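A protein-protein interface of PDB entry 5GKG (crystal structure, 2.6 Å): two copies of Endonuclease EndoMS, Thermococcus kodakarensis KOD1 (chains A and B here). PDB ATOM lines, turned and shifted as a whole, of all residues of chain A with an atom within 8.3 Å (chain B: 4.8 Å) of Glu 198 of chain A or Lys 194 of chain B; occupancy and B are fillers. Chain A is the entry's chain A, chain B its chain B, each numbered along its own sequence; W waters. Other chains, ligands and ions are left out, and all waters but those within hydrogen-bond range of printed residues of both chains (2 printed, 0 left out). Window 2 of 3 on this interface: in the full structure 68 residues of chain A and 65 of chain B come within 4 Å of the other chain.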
ATOM      1  N   ILE A 159     -29.384 -24.141  -0.733  1.00  0.00           N
ATOM      2  CA  ILE A 159     -29.694 -22.758  -0.483  1.00  0.00           C
ATOM      3  C   ILE A 159     -31.090 -22.665  -1.060  1.00  0.00           C
ATOM      4  O   ILE A 159     -31.684 -23.698  -1.359  1.00  0.00           O
ATOM      5  CB  ILE A 159     -28.681 -21.815  -1.098  1.00  0.00           C
ATOM      6  CG1 ILE A 159     -28.602 -22.009  -2.616  1.00  0.00           C
ATOM      7  CG2 ILE A 159     -27.319 -22.078  -0.444  1.00  0.00           C
ATOM      8  CD1 ILE A 159     -27.609 -21.075  -3.320  1.00  0.00           C
ATOM      9  N   VAL A 177     -18.692 -19.447  -1.695  1.00  0.00           N
ATOM     10  CA  VAL A 177     -19.243 -20.568  -2.472  1.00  0.00           C
ATOM     11  C   VAL A 177     -18.128 -21.227  -3.255  1.00  0.00           C
ATOM     12  O   VAL A 177     -17.369 -20.533  -3.947  1.00  0.00           O
ATOM     13  CB  VAL A 177     -20.309 -20.133  -3.506  1.00  0.00           C
ATOM     14  CG1 VAL A 177     -21.007 -21.344  -4.087  1.00  0.00           C
ATOM     15  CG2 VAL A 177     -21.283 -19.238  -2.895  1.00  0.00           C
ATOM     16  N   VAL A 190     -19.783 -22.426 -14.502  1.00  0.00           N
ATOM     17  CA  VAL A 190     -19.674 -21.040 -14.093  1.00  0.00           C
ATOM     18  C   VAL A 190     -21.078 -20.482 -13.885  1.00  0.00           C
ATOM     19  O   VAL A 190     -21.308 -19.693 -12.968  1.00  0.00           O
ATOM     20  CB  VAL A 190     -18.901 -20.193 -15.107  1.00  0.00           C
ATOM     21  CG1 VAL A 190     -18.873 -18.794 -14.641  1.00  0.00           C
ATOM     22  CG2 VAL A 190     -17.461 -20.691 -15.232  1.00  0.00           C
ATOM     23  N   ARG A 191     -22.014 -20.939 -14.711  1.00  0.00           N
ATOM     24  CA  ARG A 191     -23.429 -20.600 -14.586  1.00  0.00           C
ATOM     25  C   ARG A 191     -24.003 -21.065 -13.244  1.00  0.00           C
ATOM     26  O   ARG A 191     -24.777 -20.342 -12.613  1.00  0.00           O
ATOM     27  CB  ARG A 191     -24.241 -21.222 -15.730  1.00  0.00           C
ATOM     28  CG  ARG A 191     -23.982 -20.620 -17.083  1.00  0.00           C
ATOM     29  CD  ARG A 191     -25.133 -20.902 -18.033  1.00  0.00           C
ATOM     30  NE  ARG A 191     -24.672 -20.686 -19.386  1.00  0.00           N
ATOM     31  CZ  ARG A 191     -24.270 -21.647 -20.215  1.00  0.00           C
ATOM     32  NH1 ARG A 191     -24.322 -22.930 -19.860  1.00  0.00           N
ATOM     33  NH2 ARG A 191     -23.848 -21.320 -21.424  1.00  0.00           N
ATOM     34  N   GLN A 192     -23.629 -22.276 -12.828  1.00  0.00           N
ATOM     35  CA  GLN A 192     -23.978 -22.792 -11.509  1.00  0.00           C
ATOM     36  C   GLN A 192     -23.427 -21.835 -10.435  1.00  0.00           C
ATOM     37  O   GLN A 192     -24.189 -21.311  -9.616  1.00  0.00           O
ATOM     38  CB  GLN A 192     -23.407 -24.204 -11.312  1.00  0.00           C
ATOM     39  CG  GLN A 192     -24.403 -25.358 -11.160  1.00  0.00           C
ATOM     40  CD  GLN A 192     -23.692 -26.712 -11.064  1.00  0.00           C
ATOM     41  OE1 GLN A 192     -23.494 -27.312  -9.961  1.00  0.00           O
ATOM     42  NE2 GLN A 192     -23.274 -27.188 -12.219  1.00  0.00           N
ATOM     43  N   LEU A 193     -22.109 -21.613 -10.469  1.00  0.00           N
ATOM     44  CA  LEU A 193     -21.415 -20.726  -9.534  1.00  0.00           C
ATOM     45  C   LEU A 193     -22.042 -19.324  -9.447  1.00  0.00           C
ATOM     46  O   LEU A 193     -22.359 -18.862  -8.358  1.00  0.00           O
ATOM     47  CB  LEU A 193     -19.937 -20.599  -9.914  1.00  0.00           C
ATOM     48  CG  LEU A 193     -19.094 -19.787  -8.926  1.00  0.00           C
ATOM     49  CD1 LEU A 193     -19.358 -20.204  -7.485  1.00  0.00           C
ATOM     50  CD2 LEU A 193     -17.602 -19.893  -9.223  1.00  0.00           C
ATOM     51  N   LYS A 194     -22.215 -18.664 -10.593  1.00  0.00           N
ATOM     52  CA  LYS A 194     -22.779 -17.320 -10.646  1.00  0.00           C
ATOM     53  C   LYS A 194     -24.158 -17.318 -10.001  1.00  0.00           C
ATOM     54  O   LYS A 194     -24.501 -16.431  -9.214  1.00  0.00           O
ATOM     55  CB  LYS A 194     -22.856 -16.830 -12.100  1.00  0.00           C
ATOM     56  CG  LYS A 194     -23.446 -15.439 -12.314  1.00  0.00           C
ATOM     57  CD  LYS A 194     -23.563 -15.142 -13.816  1.00  0.00           C
ATOM     58  CE  LYS A 194     -24.076 -13.741 -14.132  1.00  0.00           C
ATOM     59  NZ  LYS A 194     -25.531 -13.610 -14.014  1.00  0.00           N
ATOM     60  N   SER A 195     -24.933 -18.340 -10.329  1.00  0.00           N
ATOM     61  CA  SER A 195     -26.292 -18.457  -9.844  1.00  0.00           C
ATOM     62  C   SER A 195     -26.378 -18.486  -8.307  1.00  0.00           C
ATOM     63  O   SER A 195     -27.219 -17.791  -7.696  1.00  0.00           O
ATOM     64  CB  SER A 195     -26.929 -19.712 -10.426  1.00  0.00           C
ATOM     65  OG  SER A 195     -28.245 -19.911  -9.940  1.00  0.00           O
ATOM     66  N   TYR A 196     -25.505 -19.289  -7.700  1.00  0.00           N
ATOM     67  CA  TYR A 196     -25.471 -19.467  -6.249  1.00  0.00           C
ATOM     68  C   TYR A 196     -24.996 -18.189  -5.566  1.00  0.00           C
ATOM     69  O   TYR A 196     -25.580 -17.740  -4.579  1.00  0.00           O
ATOM     70  CB  TYR A 196     -24.551 -20.634  -5.849  1.00  0.00           C
ATOM     71  CG  TYR A 196     -24.904 -21.966  -6.477  1.00  0.00           C
ATOM     72  CD1 TYR A 196     -26.229 -22.296  -6.775  1.00  0.00           C
ATOM     73  CD2 TYR A 196     -23.909 -22.896  -6.766  1.00  0.00           C
ATOM     74  CE1 TYR A 196     -26.552 -23.517  -7.355  1.00  0.00           C
ATOM     75  CE2 TYR A 196     -24.214 -24.110  -7.335  1.00  0.00           C
ATOM     76  CZ  TYR A 196     -25.526 -24.420  -7.640  1.00  0.00           C
ATOM     77  OH  TYR A 196     -25.804 -25.642  -8.213  1.00  0.00           O
ATOM     78  N   VAL A 197     -23.924 -17.618  -6.099  1.00  0.00           N
ATOM     79  CA  VAL A 197     -23.337 -16.421  -5.535  1.00  0.00           C
ATOM     80  C   VAL A 197     -24.358 -15.285  -5.532  1.00  0.00           C
ATOM     81  O   VAL A 197     -24.473 -14.550  -4.558  1.00  0.00           O
ATOM     82  CB  VAL A 197     -22.080 -16.015  -6.309  1.00  0.00           C
ATOM     83  CG1 VAL A 197     -21.735 -14.540  -6.084  1.00  0.00           C
ATOM     84  CG2 VAL A 197     -20.928 -16.912  -5.918  1.00  0.00           C
ATOM     85  N   GLU A 198     -25.123 -15.158  -6.607  1.00  0.00           N
ATOM     86  CA  GLU A 198     -26.128 -14.107  -6.659  1.00  0.00           C
ATOM     87  C   GLU A 198     -27.208 -14.362  -5.608  1.00  0.00           C
ATOM     88  O   GLU A 198     -27.585 -13.446  -4.869  1.00  0.00           O
ATOM     89  CB  GLU A 198     -26.734 -13.996  -8.063  1.00  0.00           C
ATOM     90  CG  GLU A 198     -25.845 -13.209  -9.015  1.00  0.00           C
ATOM     91  CD  GLU A 198     -26.263 -13.334 -10.465  1.00  0.00           C
ATOM     92  OE1 GLU A 198     -27.400 -13.803 -10.701  1.00  0.00           O
ATOM     93  OE2 GLU A 198     -25.451 -12.970 -11.358  1.00  0.00           O
ATOM     94  N   ILE A 199     -27.681 -15.601  -5.515  1.00  0.00           N
ATOM     95  CA  ILE A 199     -28.648 -15.957  -4.476  1.00  0.00           C
ATOM     96  C   ILE A 199     -28.127 -15.662  -3.067  1.00  0.00           C
ATOM     97  O   ILE A 199     -28.865 -15.157  -2.220  1.00  0.00           O
ATOM     98  CB  ILE A 199     -29.032 -17.435  -4.562  1.00  0.00           C
ATOM     99  CG1 ILE A 199     -29.911 -17.683  -5.781  1.00  0.00           C
ATOM    100  CG2 ILE A 199     -29.768 -17.880  -3.307  1.00  0.00           C
ATOM    101  CD1 ILE A 199     -29.847 -19.103  -6.230  1.00  0.00           C
ATOM    102  N   LEU A 200     -26.854 -15.955  -2.818  1.00  0.00           N
ATOM    103  CA  LEU A 200     -26.277 -15.671  -1.513  1.00  0.00           C
ATOM    104  C   LEU A 200     -26.112 -14.179  -1.279  1.00  0.00           C
ATOM    105  O   LEU A 200     -26.331 -13.721  -0.172  1.00  0.00           O
ATOM    106  CB  LEU A 200     -24.945 -16.388  -1.345  1.00  0.00           C
ATOM    107  CG  LEU A 200     -25.276 -17.837  -0.989  1.00  0.00           C
ATOM    108  CD1 LEU A 200     -24.082 -18.722  -1.112  1.00  0.00           C
ATOM    109  CD2 LEU A 200     -25.831 -17.911   0.417  1.00  0.00           C
ATOM    110  N   ARG A 201     -25.741 -13.425  -2.313  1.00  0.00           N
ATOM    111  CA  ARG A 201     -25.677 -11.962  -2.217  1.00  0.00           C
ATOM    112  C   ARG A 201     -27.022 -11.356  -1.796  1.00  0.00           C
ATOM    113  O   ARG A 201     -27.054 -10.347  -1.100  1.00  0.00           O
ATOM    114  CB  ARG A 201     -25.237 -11.332  -3.541  1.00  0.00           C
ATOM    115  CG  ARG A 201     -23.747 -11.414  -3.828  1.00  0.00           C
ATOM    116  CD  ARG A 201     -23.312 -10.302  -4.772  1.00  0.00           C
ATOM    117  NE  ARG A 201     -22.241 -10.716  -5.671  1.00  0.00           N
ATOM    118  CZ  ARG A 201     -21.029 -11.086  -5.261  1.00  0.00           C
ATOM    119  NH1 ARG A 201     -20.756 -11.118  -3.960  1.00  0.00           N
ATOM    120  NH2 ARG A 201     -20.095 -11.445  -6.148  1.00  0.00           N
ATOM    121  N   GLU A 202     -28.127 -11.968  -2.205  1.00  0.00           N
ATOM    122  CA  GLU A 202     -29.440 -11.464  -1.826  1.00  0.00           C
ATOM    123  C   GLU A 202     -29.587 -11.389  -0.306  1.00  0.00           C
ATOM    124  O   GLU A 202     -30.151 -10.417   0.205  1.00  0.00           O
ATOM    125  CB  GLU A 202     -30.565 -12.323  -2.426  1.00  0.00           C
ATOM    126  CG  GLU A 202     -31.118 -11.786  -3.751  1.00  0.00           C
ATOM    127  CD  GLU A 202     -32.182 -12.687  -4.367  1.00  0.00           C
ATOM    128  OE1 GLU A 202     -32.694 -12.352  -5.460  1.00  0.00           O
ATOM    129  OE2 GLU A 202     -32.509 -13.731  -3.760  1.00  0.00           O
ATOM    130  N   GLU A 203     -29.115 -12.410   0.410  1.00  0.00           N
ATOM    131  CA  GLU A 203     -29.176 -12.401   1.872  1.00  0.00           C
ATOM    132  C   GLU A 203     -28.028 -11.638   2.539  1.00  0.00           C
ATOM    133  O   GLU A 203     -28.253 -10.837   3.435  1.00  0.00           O
ATOM    134  CB  GLU A 203     -29.234 -13.838   2.406  1.00  0.00           C
ATOM    135  CG  GLU A 203     -29.439 -13.942   3.924  1.00  0.00           C
ATOM    136  CD  GLU A 203     -30.899 -14.160   4.352  1.00  0.00           C
ATOM    137  OE1 GLU A 203     -31.781 -14.264   3.470  1.00  0.00           O
ATOM    138  OE2 GLU A 203     -31.160 -14.236   5.579  1.00  0.00           O
ATOM    139  N   TYR A 204     -26.800 -11.910   2.126  1.00  0.00           N
ATOM    140  CA  TYR A 204     -25.612 -11.405   2.833  1.00  0.00           C
ATOM    141  C   TYR A 204     -24.943 -10.209   2.163  1.00  0.00           C
ATOM    142  O   TYR A 204     -23.911  -9.724   2.627  1.00  0.00           O
ATOM    143  CB  TYR A 204     -24.595 -12.552   3.028  1.00  0.00           C
ATOM    144  CG  TYR A 204     -25.214 -13.677   3.805  1.00  0.00           C
ATOM    145  CD1 TYR A 204     -25.263 -13.641   5.183  1.00  0.00           C
ATOM    146  CD2 TYR A 204     -25.813 -14.744   3.162  1.00  0.00           C
ATOM    147  CE1 TYR A 204     -25.863 -14.658   5.905  1.00  0.00           C
ATOM    148  CE2 TYR A 204     -26.409 -15.762   3.873  1.00  0.00           C
ATOM    149  CZ  TYR A 204     -26.433 -15.711   5.244  1.00  0.00           C
ATOM    150  OH  TYR A 204     -27.033 -16.715   5.959  1.00  0.00           O
ATOM    151  N   GLY A 205     -25.502  -9.754   1.054  1.00  0.00           N
ATOM    152  CA  GLY A 205     -24.935  -8.603   0.375  1.00  0.00           C
ATOM    153  C   GLY A 205     -23.559  -8.858  -0.198  1.00  0.00           C
ATOM    154  O   GLY A 205     -23.139 -10.001  -0.340  1.00  0.00           O
ATOM    155  N   VAL A 208     -20.056 -11.790  -0.490  1.00  0.00           N
ATOM    156  CA  VAL A 208     -19.923 -13.160  -0.976  1.00  0.00           C
ATOM    157  C   VAL A 208     -18.900 -13.333  -2.112  1.00  0.00           C
ATOM    158  O   VAL A 208     -18.878 -12.557  -3.061  1.00  0.00           O
ATOM    159  CB  VAL A 208     -21.273 -13.678  -1.438  1.00  0.00           C
ATOM    160  CG1 VAL A 208     -21.238 -15.186  -1.593  1.00  0.00           C
ATOM    161  CG2 VAL A 208     -22.320 -13.302  -0.426  1.00  0.00           C
ATOM    162  N   ARG A 209     -18.050 -14.352  -1.991  1.00  0.00           N
ATOM    163  CA  ARG A 209     -17.087 -14.736  -3.041  1.00  0.00           C
ATOM    164  C   ARG A 209     -17.436 -16.087  -3.678  1.00  0.00           C
ATOM    165  O   ARG A 209     -17.896 -17.005  -2.992  1.00  0.00           O
ATOM    166  CB  ARG A 209     -15.675 -14.820  -2.490  1.00  0.00           C
ATOM    167  CG  ARG A 209     -15.078 -13.523  -2.055  1.00  0.00           C
ATOM    168  CD  ARG A 209     -13.846 -13.817  -1.189  1.00  0.00           C
ATOM    169  NE  ARG A 209     -12.852 -14.562  -1.944  1.00  0.00           N
ATOM    170  CZ  ARG A 209     -11.901 -15.322  -1.410  1.00  0.00           C
ATOM    171  NH1 ARG A 209     -11.820 -15.451  -0.099  1.00  0.00           N
ATOM    172  NH2 ARG A 209     -11.037 -15.968  -2.196  1.00  0.00           N
ATOM    173  N   GLY A 210     -17.345 -16.167  -5.003  1.00  0.00           N
ATOM    174  CA  GLY A 210     -17.462 -17.443  -5.683  1.00  0.00           C
ATOM    175  C   GLY A 210     -16.111 -17.952  -6.095  1.00  0.00           C
ATOM    176  O   GLY A 210     -15.304 -17.201  -6.643  1.00  0.00           O
ATOM    177  N   GLU A 228     -17.600 -11.885 -14.639  1.00  0.00           N
ATOM    178  CA  GLU A 228     -18.384 -11.706 -13.419  1.00  0.00           C
ATOM    179  C   GLU A 228     -17.498 -11.518 -12.180  1.00  0.00           C
ATOM    180  O   GLU A 228     -17.982 -11.511 -11.069  1.00  0.00           O
ATOM    181  CB  GLU A 228     -19.328 -12.896 -13.212  1.00  0.00           C
ATOM    182  CG  GLU A 228     -20.505 -12.959 -14.184  1.00  0.00           C
ATOM    183  CD  GLU A 228     -21.485 -11.807 -14.025  1.00  0.00           C
ATOM    184  OE1 GLU A 228     -21.894 -11.247 -15.066  1.00  0.00           O
ATOM    185  OE2 GLU A 228     -21.875 -11.474 -12.874  1.00  0.00           O
ATOM    186  N   LEU A 230     -15.546 -13.759 -10.790  1.00  0.00           N
ATOM    187  CA  LEU A 230     -15.483 -14.907  -9.903  1.00  0.00           C
ATOM    188  C   LEU A 230     -14.052 -15.456  -9.922  1.00  0.00           C
ATOM    189  O   LEU A 230     -13.218 -14.985 -10.697  1.00  0.00           O
ATOM    190  CB  LEU A 230     -16.501 -15.951 -10.320  1.00  0.00           C
ATOM    191  CG  LEU A 230     -17.916 -15.429 -10.128  1.00  0.00           C
ATOM    192  CD1 LEU A 230     -18.950 -16.364 -10.726  1.00  0.00           C
ATOM    193  CD2 LEU A 230     -18.153 -15.256  -8.641  1.00  0.00           C
ATOM    194  N   VAL B 190     -33.252 -22.974 -16.785  1.00  0.00           N
ATOM    195  CA  VAL B 190     -33.470 -21.559 -16.505  1.00  0.00           C
ATOM    196  C   VAL B 190     -32.153 -20.808 -16.390  1.00  0.00           C
ATOM    197  O   VAL B 190     -32.033 -19.679 -16.847  1.00  0.00           O
ATOM    198  CB  VAL B 190     -34.291 -21.341 -15.225  1.00  0.00           C
ATOM    199  CG1 VAL B 190     -34.322 -19.865 -14.869  1.00  0.00           C
ATOM    200  CG2 VAL B 190     -35.702 -21.850 -15.409  1.00  0.00           C
ATOM    201  N   ARG B 191     -31.148 -21.443 -15.816  1.00  0.00           N
ATOM    202  CA  ARG B 191     -29.837 -20.815 -15.775  1.00  0.00           C
ATOM    203  C   ARG B 191     -29.250 -20.575 -17.156  1.00  0.00           C
ATOM    204  O   ARG B 191     -28.595 -19.560 -17.353  1.00  0.00           O
ATOM    205  CB  ARG B 191     -28.854 -21.633 -14.963  1.00  0.00           C
ATOM    206  CG  ARG B 191     -29.045 -21.546 -13.463  1.00  0.00           C
ATOM    207  CD  ARG B 191     -27.958 -22.341 -12.726  1.00  0.00           C
ATOM    208  NE  ARG B 191     -28.510 -22.804 -11.467  1.00  0.00           N
ATOM    209  CZ  ARG B 191     -28.609 -24.076 -11.103  1.00  0.00           C
ATOM    210  NH1 ARG B 191     -28.140 -25.051 -11.879  1.00  0.00           N
ATOM    211  NH2 ARG B 191     -29.168 -24.357  -9.942  1.00  0.00           N
ATOM    212  N   GLN B 192     -29.466 -21.491 -18.102  1.00  0.00           N
ATOM    213  CA  GLN B 192     -29.014 -21.261 -19.473  1.00  0.00           C
ATOM    214  C   GLN B 192     -29.650 -19.959 -19.977  1.00  0.00           C
ATOM    215  O   GLN B 192     -28.940 -19.004 -20.334  1.00  0.00           O
ATOM    216  CB  GLN B 192     -29.388 -22.419 -20.418  1.00  0.00           C
ATOM    217  CG  GLN B 192     -28.629 -23.696 -20.216  1.00  0.00           C
ATOM    218  CD  GLN B 192     -28.712 -24.684 -21.389  1.00  0.00           C
ATOM    219  OE1 GLN B 192     -29.094 -24.366 -22.535  1.00  0.00           O
ATOM    220  NE2 GLN B 192     -28.414 -25.917 -21.072  1.00  0.00           N
ATOM    221  N   LEU B 193     -30.987 -19.938 -19.963  1.00  0.00           N
ATOM    222  CA  LEU B 193     -31.795 -18.829 -20.466  1.00  0.00           C
ATOM    223  C   LEU B 193     -31.409 -17.507 -19.830  1.00  0.00           C
ATOM    224  O   LEU B 193     -31.158 -16.527 -20.530  1.00  0.00           O
ATOM    225  CB  LEU B 193     -33.276 -19.102 -20.216  1.00  0.00           C
ATOM    226  CG  LEU B 193     -34.313 -18.101 -20.742  1.00  0.00           C
ATOM    227  CD1 LEU B 193     -34.236 -17.941 -22.270  1.00  0.00           C
ATOM    228  CD2 LEU B 193     -35.730 -18.525 -20.319  1.00  0.00           C
ATOM    229  N   LYS B 194     -31.367 -17.496 -18.502  1.00  0.00           N
ATOM    230  CA  LYS B 194     -31.010 -16.307 -17.758  1.00  0.00           C
ATOM    231  C   LYS B 194     -29.662 -15.785 -18.238  1.00  0.00           C
ATOM    232  O   LYS B 194     -29.487 -14.593 -18.503  1.00  0.00           O
ATOM    233  CB  LYS B 194     -30.984 -16.618 -16.265  1.00  0.00           C
ATOM    234  CG  LYS B 194     -30.181 -15.646 -15.417  1.00  0.00           C
ATOM    235  CD  LYS B 194     -30.743 -15.625 -14.002  1.00  0.00           C
ATOM    236  CE  LYS B 194     -30.086 -14.566 -13.142  1.00  0.00           C
ATOM    237  NZ  LYS B 194     -28.646 -14.873 -12.832  1.00  0.00           N
ATOM    238  N   SER B 195     -28.718 -16.705 -18.370  1.00  0.00           N
ATOM    239  CA  SER B 195     -27.376 -16.379 -18.811  1.00  0.00           C
ATOM    240  C   SER B 195     -27.381 -15.725 -20.192  1.00  0.00           C
ATOM    241  O   SER B 195     -26.690 -14.747 -20.417  1.00  0.00           O
ATOM    242  CB  SER B 195     -26.523 -17.635 -18.838  1.00  0.00           C
ATOM    243  OG  SER B 195     -25.214 -17.335 -19.227  1.00  0.00           O
ATOM    244  N   TYR B 196     -28.173 -16.270 -21.109  1.00  0.00           N
ATOM    245  CA  TYR B 196     -28.237 -15.746 -22.469  1.00  0.00           C
ATOM    246  C   TYR B 196     -28.892 -14.361 -22.487  1.00  0.00           C
ATOM    247  O   TYR B 196     -28.348 -13.423 -23.062  1.00  0.00           O
ATOM    248  CB  TYR B 196     -29.002 -16.699 -23.392  1.00  0.00           C
ATOM    249  CG  TYR B 196     -28.443 -18.108 -23.454  1.00  0.00           C
ATOM    250  CD1 TYR B 196     -27.090 -18.360 -23.270  1.00  0.00           C
ATOM    251  CD2 TYR B 196     -29.279 -19.189 -23.701  1.00  0.00           C
ATOM    252  CE1 TYR B 196     -26.593 -19.640 -23.325  1.00  0.00           C
ATOM    253  CE2 TYR B 196     -28.797 -20.458 -23.758  1.00  0.00           C
ATOM    254  CZ  TYR B 196     -27.455 -20.690 -23.571  1.00  0.00           C
ATOM    255  OH  TYR B 196     -27.001 -21.982 -23.632  1.00  0.00           O
ATOM    256  N   VAL B 197     -30.059 -14.254 -21.854  1.00  0.00           N
ATOM    257  CA  VAL B 197     -30.786 -12.996 -21.749  1.00  0.00           C
ATOM    258  C   VAL B 197     -29.939 -11.850 -21.175  1.00  0.00           C
ATOM    259  O   VAL B 197     -29.899 -10.753 -21.720  1.00  0.00           O
ATOM    260  CB  VAL B 197     -32.019 -13.182 -20.894  1.00  0.00           C
ATOM    261  CG1 VAL B 197     -32.604 -11.818 -20.503  1.00  0.00           C
ATOM    262  CG2 VAL B 197     -33.031 -14.055 -21.647  1.00  0.00           C
ATOM    263  N   GLU B 198     -29.241 -12.117 -20.084  1.00  0.00           N
ATOM    264  CA  GLU B 198     -28.351 -11.127 -19.513  1.00  0.00           C
ATOM    265  C   GLU B 198     -27.311 -10.629 -20.516  1.00  0.00           C
ATOM    266  O   GLU B 198     -27.054  -9.429 -20.613  1.00  0.00           O
ATOM    267  CB  GLU B 198     -27.653 -11.701 -18.284  1.00  0.00           C
ATOM    268  CG  GLU B 198     -28.579 -11.837 -17.100  1.00  0.00           C
ATOM    269  CD  GLU B 198     -27.906 -12.441 -15.885  1.00  0.00           C
ATOM    270  OE1 GLU B 198     -26.759 -12.936 -15.997  1.00  0.00           O
ATOM    271  OE2 GLU B 198     -28.534 -12.417 -14.809  1.00  0.00           O
ATOM    272  N   GLU B 228     -36.727 -13.920 -12.016  1.00  0.00           N
ATOM    273  CA  GLU B 228     -35.872 -13.264 -13.006  1.00  0.00           C
ATOM    274  C   GLU B 228     -36.655 -12.520 -14.087  1.00  0.00           C
ATOM    275  O   GLU B 228     -36.062 -11.893 -14.975  1.00  0.00           O
ATOM    276  CB  GLU B 228     -34.944 -14.288 -13.661  1.00  0.00           C
ATOM    277  CG  GLU B 228     -33.924 -14.868 -12.708  1.00  0.00           C
ATOM    278  CD  GLU B 228     -33.154 -13.801 -11.942  1.00  0.00           C
ATOM    279  OE1 GLU B 228     -32.855 -12.734 -12.523  1.00  0.00           O
ATOM    280  OE2 GLU B 228     -32.844 -14.035 -10.751  1.00  0.00           O
ATOM    281  N   LEU B 230     -38.635 -14.023 -16.309  1.00  0.00           N
ATOM    282  CA  LEU B 230     -38.598 -14.745 -17.555  1.00  0.00           C
ATOM    283  C   LEU B 230     -39.944 -15.392 -17.751  1.00  0.00           C
ATOM    284  O   LEU B 230     -40.775 -15.391 -16.855  1.00  0.00           O
ATOM    285  CB  LEU B 230     -37.481 -15.766 -17.526  1.00  0.00           C
ATOM    286  CG  LEU B 230     -36.142 -15.055 -17.420  1.00  0.00           C
ATOM    287  CD1 LEU B 230     -35.002 -15.988 -17.007  1.00  0.00           C
ATOM    288  CD2 LEU B 230     -35.879 -14.501 -18.774  1.00  0.00           C
HETATM  289  O   HOH W   1     -29.324 -21.963  -8.695  1.00  0.00           O
HETATM  290  O   HOH W   2     -28.880 -16.228 -10.015  1.00  0.00           O
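The guanidinium group (NE) of Arg 191 of chain A lies within hydrogen-bond range of the side-chain hydroxyl (OG) of Ser 195 of chain B (3.4 Å). NZ of Lys 194 of chain A lies within salt-bridge range of OE1 of Glu 198 of chain B, at 2.4 Å. OG of Ser 195 of chain A is in hydrogen-bond range of NE of Arg 191 of chain B, 3.3 Å away. The side-chain carboxylate (OE1) of Glu 198 of chain A is in salt-bridge range of the side-chain amino group (NZ) of Lys 194 of chain B (2.7 Å).
The side-chain amide oxygen (OE1) of Gln 192 of chain A lies close to the side-chain hydroxyl (OH) of Tyr 196 of chain A (3.3 Å). The side-chain amino group (NZ) of Lys 194 of chain A lies within salt-bridge range of the side-chain carboxylate (OE2) of Glu 198 of chain A, 2.7 Å away. OE1 of Gln 192 of chain B is in hydrogen-bond range of OH of Tyr 196 of chain B (3.4 Å). OE2 of Glu 198 of chain B is in salt-bridge range of NZ of Lys 194 of chain B, at 3.2 Å.
Among the printed residues, pairs that only touch across the chains: Arg 191 of chain A with Arg 191 of chain B, Arg 191 of chain A with Tyr 196 of chain B, Gln 192 of chain A with Arg 191 of chain B, Lys 194 of chain A with Lys 194 of chain B and Tyr 196 of chain A with Arg 191 of chain B.
Lys 194 of chain B touches just these residues of chain A: Lys 194 (3.6 Å) and Glu 198 (2.7 Å). Of the printed residues of chain B, Gln 192 of chain A touches Arg 191. Of the printed residues of chain B, Lys 194 of chain A touches Lys 194 and Glu 198. Printed residues of chain A within 4 Å of Glu 198 of chain B: Lys 194. Glu 203 of chain A touches none of the printed residues of chain B. The nearest residue of chain A that does not touch Lys 194 of chain B is Ser 195 of chain A (5.2 Å). The nearest printed residue of chain B that does not touch Arg 191 of chain A is Gln 192 of chain B (4.2 Å).
Of the 11 printed residues of chain B, 5 touch a printed residue of chain A. Printed residues of chain B that touch a printed residue of chain A: Arg 191, Lys 194, Ser 195, Tyr 196 and Glu 198. Hydrophobic or aromatic side chains of chain B within 4 Å of the printed part of chain A: Tyr 196. Among the printed residues, 9 pairs touch across the chains. Among the printed residues, Asp or Glu carboxylates within 4 Å of a Lys or Arg side-chain nitrogen of the other chain: Lys 194 of chain A with Glu 198 of chain B and Glu 198 of chain A with Lys 194 of chain B.
Arg 191 of chain A touches Ser 195 of chain B, and with the chains exchanged Ser 195 of chain A touches Arg 191 of chain B. Arg 191 of chain A touches Tyr 196 of chain B, and with the chains exchanged Tyr 196 of chain A touches Arg 191 of chain B. Lys 194 of chain B touches its own counterpart, Lys 194 of chain A. Lys 194 of chain A touches Glu 198 of chain B, and with the chains exchanged Glu 198 of chain A touches Lys 194 of chain B. Positions printed for both chains: 190, 191, 192, 193, 194, 195, 196, 197, 198, 228 and 230. Of the 9 pairs that touch across the chains among the printed residues, 8 have their exchanged pair printed and touching as well.
Water W1 lies within hydrogen-bond range of the side-chain hydroxyl (OG) of Ser 195 of chain A and the guanidinium group (NH2) of Arg 191 of chain B. Water W2 lies within hydrogen-bond range of OE1 of Glu 198 of chain A (2.9 Å), NZ of Lys 194 of chain B (3.1 Å) and O of Ser 195 of chain A (3.3 Å).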
